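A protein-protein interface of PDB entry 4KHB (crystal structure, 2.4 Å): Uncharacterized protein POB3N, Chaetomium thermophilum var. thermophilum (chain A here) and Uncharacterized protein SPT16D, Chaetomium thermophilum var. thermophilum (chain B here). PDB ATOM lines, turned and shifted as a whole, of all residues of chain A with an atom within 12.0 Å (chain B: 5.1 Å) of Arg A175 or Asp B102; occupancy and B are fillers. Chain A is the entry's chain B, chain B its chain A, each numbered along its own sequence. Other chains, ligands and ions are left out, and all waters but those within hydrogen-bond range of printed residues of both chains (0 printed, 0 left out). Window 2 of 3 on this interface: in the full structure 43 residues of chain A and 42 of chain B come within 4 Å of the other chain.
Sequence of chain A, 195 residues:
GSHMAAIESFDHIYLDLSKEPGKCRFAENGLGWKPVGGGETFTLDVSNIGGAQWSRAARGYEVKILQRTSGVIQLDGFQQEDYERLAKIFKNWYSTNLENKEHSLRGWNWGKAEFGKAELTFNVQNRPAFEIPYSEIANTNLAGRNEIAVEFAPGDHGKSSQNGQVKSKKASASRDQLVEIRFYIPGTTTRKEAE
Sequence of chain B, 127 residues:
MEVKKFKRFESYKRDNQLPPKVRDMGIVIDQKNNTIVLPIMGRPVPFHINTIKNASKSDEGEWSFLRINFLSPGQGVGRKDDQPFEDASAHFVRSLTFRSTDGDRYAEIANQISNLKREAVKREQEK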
ATOM      1  N   LEU A  17      25.829 -14.145 -14.694  1.00  0.00           N
ATOM      2  CA  LEU A  17      24.554 -14.314 -15.394  1.00  0.00           C
ATOM      3  C   LEU A  17      23.971 -12.979 -15.827  1.00  0.00           C
ATOM      4  O   LEU A  17      22.751 -12.801 -15.846  1.00  0.00           O
ATOM      5  CB  LEU A  17      23.536 -15.107 -14.559  1.00  0.00           C
ATOM      6  CG  LEU A  17      24.019 -16.412 -13.923  1.00  0.00           C
ATOM      7  CD1 LEU A  17      22.848 -17.253 -13.431  1.00  0.00           C
ATOM      8  CD2 LEU A  17      24.872 -17.192 -14.891  1.00  0.00           C
ATOM      9  N   SER A  18      24.848 -12.042 -16.173  1.00  0.00           N
ATOM     10  CA  SER A  18      24.403 -10.760 -16.693  1.00  0.00           C
ATOM     11  C   SER A  18      23.632 -10.986 -17.984  1.00  0.00           C
ATOM     12  O   SER A  18      23.969 -11.862 -18.782  1.00  0.00           O
ATOM     13  CB  SER A  18      25.591  -9.827 -16.937  1.00  0.00           C
ATOM     14  OG  SER A  18      26.431 -10.319 -17.964  1.00  0.00           O
ATOM     15  N   LYS A  19      22.586 -10.197 -18.175  1.00  0.00           N
ATOM     16  CA  LYS A  19      21.806 -10.243 -19.399  1.00  0.00           C
ATOM     17  C   LYS A  19      22.572  -9.626 -20.563  1.00  0.00           C
ATOM     18  O   LYS A  19      22.387 -10.016 -21.715  1.00  0.00           O
ATOM     19  CB  LYS A  19      20.451  -9.552 -19.195  1.00  0.00           C
ATOM     20  CG  LYS A  19      20.189  -9.081 -17.760  1.00  0.00           C
ATOM     21  CD  LYS A  19      20.904  -7.778 -17.406  1.00  0.00           C
ATOM     22  CE  LYS A  19      21.291  -7.749 -15.927  1.00  0.00           C
ATOM     23  NZ  LYS A  19      20.140  -8.000 -15.014  1.00  0.00           N
ATOM     24  N   ALA A  58      26.242 -22.379 -20.411  1.00  0.00           N
ATOM     25  CA  ALA A  58      25.239 -21.955 -21.381  1.00  0.00           C
ATOM     26  C   ALA A  58      25.837 -21.005 -22.414  1.00  0.00           C
ATOM     27  O   ALA A  58      26.377 -19.955 -22.066  1.00  0.00           O
ATOM     28  CB  ALA A  58      24.062 -21.301 -20.675  1.00  0.00           C
ATOM     29  N   PRO A 154      13.738 -15.108  -5.841  1.00  0.00           N
ATOM     30  CA  PRO A 154      13.953 -14.500  -7.155  1.00  0.00           C
ATOM     31  C   PRO A 154      13.170 -13.201  -7.297  1.00  0.00           C
ATOM     32  O   PRO A 154      13.538 -12.344  -8.101  1.00  0.00           O
ATOM     33  CB  PRO A 154      13.413 -15.561  -8.116  1.00  0.00           C
ATOM     34  CG  PRO A 154      12.368 -16.276  -7.325  1.00  0.00           C
ATOM     35  CD  PRO A 154      12.915 -16.330  -5.926  1.00  0.00           C
ATOM     36  N   GLY A 155      12.098 -13.066  -6.521  1.00  0.00           N
ATOM     37  CA  GLY A 155      11.230 -11.909  -6.613  1.00  0.00           C
ATOM     38  C   GLY A 155      11.200 -11.103  -5.330  1.00  0.00           C
ATOM     39  O   GLY A 155      11.450  -9.898  -5.334  1.00  0.00           O
ATOM     40  N   SER A 168      17.888 -13.199  -4.688  1.00  0.00           N
ATOM     41  CA  SER A 168      18.598 -14.206  -5.474  1.00  0.00           C
ATOM     42  C   SER A 168      18.533 -13.680  -6.907  1.00  0.00           C
ATOM     43  O   SER A 168      17.565 -13.940  -7.625  1.00  0.00           O
ATOM     44  CB  SER A 168      17.936 -15.574  -5.299  1.00  0.00           C
ATOM     45  OG  SER A 168      17.861 -15.938  -3.931  1.00  0.00           O
ATOM     46  N   LYS A 169      19.567 -12.951  -7.321  1.00  0.00           N
ATOM     47  CA  LYS A 169      19.687 -12.478  -8.701  1.00  0.00           C
ATOM     48  C   LYS A 169      20.010 -13.556  -9.742  1.00  0.00           C
ATOM     49  O   LYS A 169      19.506 -13.497 -10.866  1.00  0.00           O
ATOM     50  CB  LYS A 169      20.674 -11.307  -8.790  1.00  0.00           C
ATOM     51  CG  LYS A 169      20.693 -10.437  -7.536  1.00  0.00           C
ATOM     52  CD  LYS A 169      21.847  -9.442  -7.526  1.00  0.00           C
ATOM     53  CE  LYS A 169      21.936  -8.715  -6.183  1.00  0.00           C
ATOM     54  NZ  LYS A 169      23.142  -9.088  -5.395  1.00  0.00           N
ATOM     55  N   LYS A 170      20.846 -14.529  -9.388  1.00  0.00           N
ATOM     56  CA  LYS A 170      21.195 -15.580 -10.343  1.00  0.00           C
ATOM     57  C   LYS A 170      20.061 -16.585 -10.520  1.00  0.00           C
ATOM     58  O   LYS A 170      19.950 -17.228 -11.564  1.00  0.00           O
ATOM     59  CB  LYS A 170      22.481 -16.306  -9.933  1.00  0.00           C
ATOM     60  CG  LYS A 170      23.739 -15.453  -9.996  1.00  0.00           C
ATOM     61  CD  LYS A 170      24.972 -16.282  -9.659  1.00  0.00           C
ATOM     62  CE  LYS A 170      26.243 -15.471  -9.846  1.00  0.00           C
ATOM     63  NZ  LYS A 170      27.470 -16.240  -9.502  1.00  0.00           N
ATOM     64  N   ALA A 171      19.222 -16.720  -9.500  1.00  0.00           N
ATOM     65  CA  ALA A 171      18.055 -17.586  -9.594  1.00  0.00           C
ATOM     66  C   ALA A 171      17.018 -17.001 -10.546  1.00  0.00           C
ATOM     67  O   ALA A 171      16.228 -17.733 -11.144  1.00  0.00           O
ATOM     68  CB  ALA A 171      17.448 -17.810  -8.218  1.00  0.00           C
ATOM     69  N   SER A 172      17.026 -15.677 -10.677  1.00  0.00           N
ATOM     70  CA  SER A 172      16.019 -14.971 -11.465  1.00  0.00           C
ATOM     71  C   SER A 172      16.555 -14.472 -12.804  1.00  0.00           C
ATOM     72  O   SER A 172      15.847 -13.783 -13.538  1.00  0.00           O
ATOM     73  CB  SER A 172      15.445 -13.796 -10.666  1.00  0.00           C
ATOM     74  OG  SER A 172      16.434 -12.816 -10.412  1.00  0.00           O
ATOM     75  N   ALA A 173      17.795 -14.824 -13.128  1.00  0.00           N
ATOM     76  CA  ALA A 173      18.409 -14.337 -14.357  1.00  0.00           C
ATOM     77  C   ALA A 173      17.809 -15.029 -15.571  1.00  0.00           C
ATOM     78  O   ALA A 173      17.797 -14.478 -16.675  1.00  0.00           O
ATOM     79  CB  ALA A 173      19.911 -14.545 -14.317  1.00  0.00           C
ATOM     80  N   SER A 174      17.316 -16.243 -15.362  1.00  0.00           N
ATOM     81  CA  SER A 174      16.689 -16.997 -16.432  1.00  0.00           C
ATOM     82  C   SER A 174      15.218 -16.622 -16.521  1.00  0.00           C
ATOM     83  O   SER A 174      14.675 -15.991 -15.612  1.00  0.00           O
ATOM     84  CB  SER A 174      16.823 -18.500 -16.170  1.00  0.00           C
ATOM     85  OG  SER A 174      16.006 -19.243 -17.057  1.00  0.00           O
ATOM     86  N   ARG A 175      14.574 -17.030 -17.610  1.00  0.00           N
ATOM     87  CA  ARG A 175      13.139 -16.854 -17.780  1.00  0.00           C
ATOM     88  C   ARG A 175      12.423 -17.816 -16.858  1.00  0.00           C
ATOM     89  O   ARG A 175      11.298 -17.569 -16.416  1.00  0.00           O
ATOM     90  CB  ARG A 175      12.740 -17.194 -19.209  1.00  0.00           C
ATOM     91  CG  ARG A 175      11.372 -16.698 -19.622  1.00  0.00           C
ATOM     92  CD  ARG A 175      11.304 -16.527 -21.122  1.00  0.00           C
ATOM     93  NE  ARG A 175      10.000 -16.951 -21.624  1.00  0.00           N
ATOM     94  CZ  ARG A 175       9.536 -16.680 -22.839  1.00  0.00           C
ATOM     95  NH1 ARG A 175      10.275 -15.991 -23.695  1.00  0.00           N
ATOM     96  NH2 ARG A 175       8.339 -17.117 -23.203  1.00  0.00           N
ATOM     97  N   ASP A 176      13.091 -18.930 -16.583  1.00  0.00           N
ATOM     98  CA  ASP A 176      12.573 -19.921 -15.662  1.00  0.00           C
ATOM     99  C   ASP A 176      13.311 -19.761 -14.348  1.00  0.00           C
ATOM    100  O   ASP A 176      14.435 -20.242 -14.191  1.00  0.00           O
ATOM    101  CB  ASP A 176      12.773 -21.328 -16.233  1.00  0.00           C
ATOM    102  CG  ASP A 176      11.978 -21.561 -17.504  1.00  0.00           C
ATOM    103  OD1 ASP A 176      10.759 -21.289 -17.503  1.00  0.00           O
ATOM    104  OD2 ASP A 176      12.574 -22.014 -18.505  1.00  0.00           O
ATOM    105  N   GLN A 177      12.670 -19.085 -13.402  1.00  0.00           N
ATOM    106  CA  GLN A 177      13.324 -18.726 -12.153  1.00  0.00           C
ATOM    107  C   GLN A 177      13.291 -19.865 -11.148  1.00  0.00           C
ATOM    108  O   GLN A 177      12.228 -20.418 -10.853  1.00  0.00           O
ATOM    109  CB  GLN A 177      12.665 -17.476 -11.558  1.00  0.00           C
ATOM    110  CG  GLN A 177      12.692 -16.266 -12.491  1.00  0.00           C
ATOM    111  CD  GLN A 177      12.040 -15.044 -11.880  1.00  0.00           C
ATOM    112  OE1 GLN A 177      11.280 -15.147 -10.917  1.00  0.00           O
ATOM    113  NE2 GLN A 177      12.335 -13.877 -12.436  1.00  0.00           N
ATOM    114  N   LEU A 178      14.459 -20.196 -10.606  1.00  0.00           N
ATOM    115  CA  LEU A 178      14.559 -21.266  -9.623  1.00  0.00           C
ATOM    116  C   LEU A 178      13.970 -20.798  -8.297  1.00  0.00           C
ATOM    117  O   LEU A 178      14.329 -19.731  -7.788  1.00  0.00           O
ATOM    118  CB  LEU A 178      16.014 -21.711  -9.447  1.00  0.00           C
ATOM    119  CG  LEU A 178      16.248 -22.918  -8.539  1.00  0.00           C
ATOM    120  CD1 LEU A 178      15.492 -24.124  -9.066  1.00  0.00           C
ATOM    121  CD2 LEU A 178      17.734 -23.236  -8.443  1.00  0.00           C
ATOM    122  N   VAL A 179      13.066 -21.600  -7.748  1.00  0.00           N
ATOM    123  CA  VAL A 179      12.339 -21.226  -6.544  1.00  0.00           C
ATOM    124  C   VAL A 179      12.816 -22.023  -5.335  1.00  0.00           C
ATOM    125  O   VAL A 179      13.014 -21.469  -4.250  1.00  0.00           O
ATOM    126  CB  VAL A 179      10.819 -21.438  -6.736  1.00  0.00           C
ATOM    127  CG1 VAL A 179      10.074 -21.172  -5.448  1.00  0.00           C
ATOM    128  CG2 VAL A 179      10.291 -20.541  -7.837  1.00  0.00           C
ATOM    129  N   MET B  25      19.222 -20.319 -21.391  1.00  0.00           N
ATOM    130  CA  MET B  25      19.006 -20.536 -19.960  1.00  0.00           C
ATOM    131  C   MET B  25      17.550 -20.852 -19.636  1.00  0.00           C
ATOM    132  O   MET B  25      17.038 -20.444 -18.594  1.00  0.00           O
ATOM    133  CB  MET B  25      19.506 -19.343 -19.131  1.00  0.00           C
ATOM    134  CG  MET B  25      20.885 -19.555 -18.526  1.00  0.00           C
ATOM    135  SD  MET B  25      21.601 -18.065 -17.808  1.00  0.00           S
ATOM    136  CE  MET B  25      22.947 -17.797 -18.960  1.00  0.00           C
ATOM    137  N   SER B  64       3.184 -18.668 -12.671  1.00  0.00           N
ATOM    138  CA  SER B  64       2.879 -20.088 -12.779  1.00  0.00           C
ATOM    139  C   SER B  64       4.048 -20.891 -12.230  1.00  0.00           C
ATOM    140  O   SER B  64       5.194 -20.447 -12.294  1.00  0.00           O
ATOM    141  CB  SER B  64       2.599 -20.470 -14.233  1.00  0.00           C
ATOM    142  OG  SER B  64       1.437 -19.814 -14.709  1.00  0.00           O
ATOM    143  N   ARG B  99       9.461 -20.928 -11.418  1.00  0.00           N
ATOM    144  CA  ARG B  99       8.313 -20.052 -11.602  1.00  0.00           C
ATOM    145  C   ARG B  99       8.470 -19.243 -12.885  1.00  0.00           C
ATOM    146  O   ARG B  99       9.586 -18.876 -13.268  1.00  0.00           O
ATOM    147  CB  ARG B  99       8.105 -19.131 -10.392  1.00  0.00           C
ATOM    148  CG  ARG B  99       9.056 -17.947 -10.333  1.00  0.00           C
ATOM    149  CD  ARG B  99       8.621 -16.939  -9.284  1.00  0.00           C
ATOM    150  NE  ARG B  99       9.301 -15.660  -9.465  1.00  0.00           N
ATOM    151  CZ  ARG B  99       9.059 -14.576  -8.738  1.00  0.00           C
ATOM    152  NH1 ARG B  99       8.152 -14.608  -7.771  1.00  0.00           N
ATOM    153  NH2 ARG B  99       9.720 -13.455  -8.983  1.00  0.00           N
ATOM    154  N   SER B 100       7.351 -18.986 -13.555  1.00  0.00           N
ATOM    155  CA  SER B 100       7.349 -18.137 -14.741  1.00  0.00           C
ATOM    156  C   SER B 100       5.979 -17.507 -14.953  1.00  0.00           C
ATOM    157  O   SER B 100       5.005 -17.876 -14.292  1.00  0.00           O
ATOM    158  CB  SER B 100       7.759 -18.940 -15.979  1.00  0.00           C
ATOM    159  OG  SER B 100       7.596 -18.176 -17.160  1.00  0.00           O
ATOM    160  N   THR B 101       5.910 -16.551 -15.874  1.00  0.00           N
ATOM    161  CA  THR B 101       4.645 -15.916 -16.227  1.00  0.00           C
ATOM    162  C   THR B 101       3.970 -16.619 -17.405  1.00  0.00           C
ATOM    163  O   THR B 101       2.788 -16.397 -17.677  1.00  0.00           O
ATOM    164  CB  THR B 101       4.823 -14.410 -16.529  1.00  0.00           C
ATOM    165  OG1 THR B 101       5.828 -14.234 -17.537  1.00  0.00           O
ATOM    166  CG2 THR B 101       5.247 -13.666 -15.269  1.00  0.00           C
ATOM    167  N   ASP B 102       4.723 -17.473 -18.095  1.00  0.00           N
ATOM    168  CA  ASP B 102       4.183 -18.228 -19.224  1.00  0.00           C
ATOM    169  C   ASP B 102       3.407 -19.445 -18.725  1.00  0.00           C
ATOM    170  O   ASP B 102       3.951 -20.548 -18.641  1.00  0.00           O
ATOM    171  CB  ASP B 102       5.300 -18.666 -20.182  1.00  0.00           C
ATOM    172  CG  ASP B 102       6.341 -17.583 -20.406  1.00  0.00           C
ATOM    173  OD1 ASP B 102       6.007 -16.390 -20.251  1.00  0.00           O
ATOM    174  OD2 ASP B 102       7.494 -17.928 -20.746  1.00  0.00           O
ATOM    175  N   GLY B 103       2.136 -19.231 -18.389  1.00  0.00           N
ATOM    176  CA  GLY B 103       1.284 -20.296 -17.889  1.00  0.00           C
ATOM    177  C   GLY B 103       1.026 -21.420 -18.873  1.00  0.00           C
ATOM    178  O   GLY B 103       0.925 -22.584 -18.482  1.00  0.00           O
ATOM    179  N   ASP B 104       0.918 -21.072 -20.151  1.00  0.00           N
ATOM    180  CA  ASP B 104       0.664 -22.064 -21.190  1.00  0.00           C
ATOM    181  C   ASP B 104       1.907 -22.885 -21.511  1.00  0.00           C
ATOM    182  O   ASP B 104       1.811 -24.070 -21.829  1.00  0.00           O
ATOM    183  CB  ASP B 104       0.114 -21.402 -22.458  1.00  0.00           C
ATOM    184  CG  ASP B 104      -1.338 -20.983 -22.316  1.00  0.00           C
ATOM    185  OD1 ASP B 104      -1.851 -20.962 -21.178  1.00  0.00           O
ATOM    186  OD2 ASP B 104      -1.964 -20.677 -23.352  1.00  0.00           O
ATOM    187  N   ARG B 105       3.074 -22.252 -21.433  1.00  0.00           N
ATOM    188  CA  ARG B 105       4.325 -22.963 -21.666  1.00  0.00           C
ATOM    189  C   ARG B 105       4.549 -24.032 -20.601  1.00  0.00           C
ATOM    190  O   ARG B 105       4.937 -25.154 -20.917  1.00  0.00           O
ATOM    191  CB  ARG B 105       5.511 -21.993 -21.712  1.00  0.00           C
ATOM    192  CG  ARG B 105       6.813 -22.628 -22.193  1.00  0.00           C
ATOM    193  CD  ARG B 105       7.858 -21.579 -22.543  1.00  0.00           C
ATOM    194  NE  ARG B 105       8.167 -20.716 -21.406  1.00  0.00           N
ATOM    195  CZ  ARG B 105       9.145 -20.946 -20.536  1.00  0.00           C
ATOM    196  NH1 ARG B 105       9.917 -22.015 -20.668  1.00  0.00           N
ATOM    197  NH2 ARG B 105       9.347 -20.107 -19.529  1.00  0.00           N
ATOM    198  N   TYR B 106       4.288 -23.687 -19.342  1.00  0.00           N
ATOM    199  CA  TYR B 106       4.476 -24.630 -18.241  1.00  0.00           C
ATOM    200  C   TYR B 106       3.453 -25.761 -18.290  1.00  0.00           C
ATOM    201  O   TYR B 106       3.729 -26.878 -17.848  1.00  0.00           O
ATOM    202  CB  TYR B 106       4.433 -23.915 -16.884  1.00  0.00           C
ATOM    203  CG  TYR B 106       5.766 -23.337 -16.449  1.00  0.00           C
ATOM    204  CD1 TYR B 106       6.861 -23.344 -17.304  1.00  0.00           C
ATOM    205  CD2 TYR B 106       5.935 -22.810 -15.175  1.00  0.00           C
ATOM    206  CE1 TYR B 106       8.078 -22.827 -16.912  1.00  0.00           C
ATOM    207  CE2 TYR B 106       7.154 -22.291 -14.771  1.00  0.00           C
ATOM    208  CZ  TYR B 106       8.221 -22.304 -15.646  1.00  0.00           C
ATOM    209  OH  TYR B 106       9.439 -21.791 -15.264  1.00  0.00           O
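Among the printed residues, merely in contact across the chains: Val A179 with Arg B99 (3.6 Å), Pro A154 with Arg B99 (3.8 Å), Arg A175 with Arg B99 (3.8 Å), Arg A175 with Ser B100 (3.8 Å), Arg A175 with Arg B105 (3.8 Å) and Asp A176 with Arg B99 (3.97 Å).
Leu A17 touches none of the printed residues of chain B.
Ser A168 touches none of the printed residues of chain B.
Printed residues of chain B within 4 Å of Ser A174: Met B25.
Arg A175 touches just these residues of chain B: Arg B99, Ser B100, Asp B102 and Arg B105.
Printed residues of chain B within 4 Å of Asp A176: Arg B99, Arg B105 and Tyr B106.
Of the printed residues of chain A, Met B25 touches Ser A174.
No residue of chain A comes within 4 Å of Thr B101.
Asp B102 touches one residue of chain A.
No residue of chain A comes within 4 Å of Gly B103.
Of chain A, only Arg A175 (3.8 Å) and Asp A176 (2.7 Å) come within 4 Å of Arg B105.
Of chain A, only Asp A176 comes within 4 Å of Tyr B106.
The nearest residue of chain B that does not touch Arg A175 is Met B25 (4.3 Å).
The nearest printed residue of chain B that does not touch Gln A177 is Tyr B106 (4.6 Å).
NE of Arg B99 sits at hydrogen-bond distance from OE1 of Gln A177 (2.5 Å).
The guanidinium group of Arg A175 is in salt-bridge range of the side-chain carboxylate of Asp B102, at 2.7 Å.
NH2 of Arg B105 lies within salt-bridge range of OD1 of Asp A176 (2.7 Å).
The side-chain carboxylate of Asp A176 sits at hydrogen-bond distance from the side-chain hydroxyl of Tyr B106 (2.6 Å).
NH2 of Arg B99 sits close to N of Gly A155 (3.4 Å).
The side-chain hydroxyl (OG) of Ser A174 sits close to the backbone carbonyl oxygen (O) of Met B25 (2.2 Å).
The backbone carbonyl oxygen (O) of Ser B100 lies within hydrogen-bond range of the backbone NH (N) of Ser B64.
The side-chain hydroxyl of Ser B100 sits at hydrogen-bond distance from the backbone NH of Asp B102.
The side-chain hydroxyl (OG1) of Thr B101 sits at hydrogen-bond distance from the side-chain carboxylate (OD1) of Asp B102, 3.5 Å away.
OD2 of Asp B102 lies within salt-bridge range of NE of Arg B105 (2.9 Å).
The side-chain hydroxyl (OG) of Ser A174 sits at hydrogen-bond distance from the backbone NH (N) of Asp A176 (3.0 Å).
Hydrophobic or aromatic side chains of chain B within 4 Å of the printed part of chain A: Tyr B106.
Printed residues of chain A that touch a printed residue of chain B: Pro A154, Gly A155, Ser A174, Arg A175, Asp A176, Gln A177 and Val A179.
Among the printed residues, Asp or Glu carboxylates within 4 Å of a Lys or Arg side-chain nitrogen of the other chain: Arg A175 with Asp B102 (2.7 Å) and Asp A176 with Arg B105 (2.7 Å).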
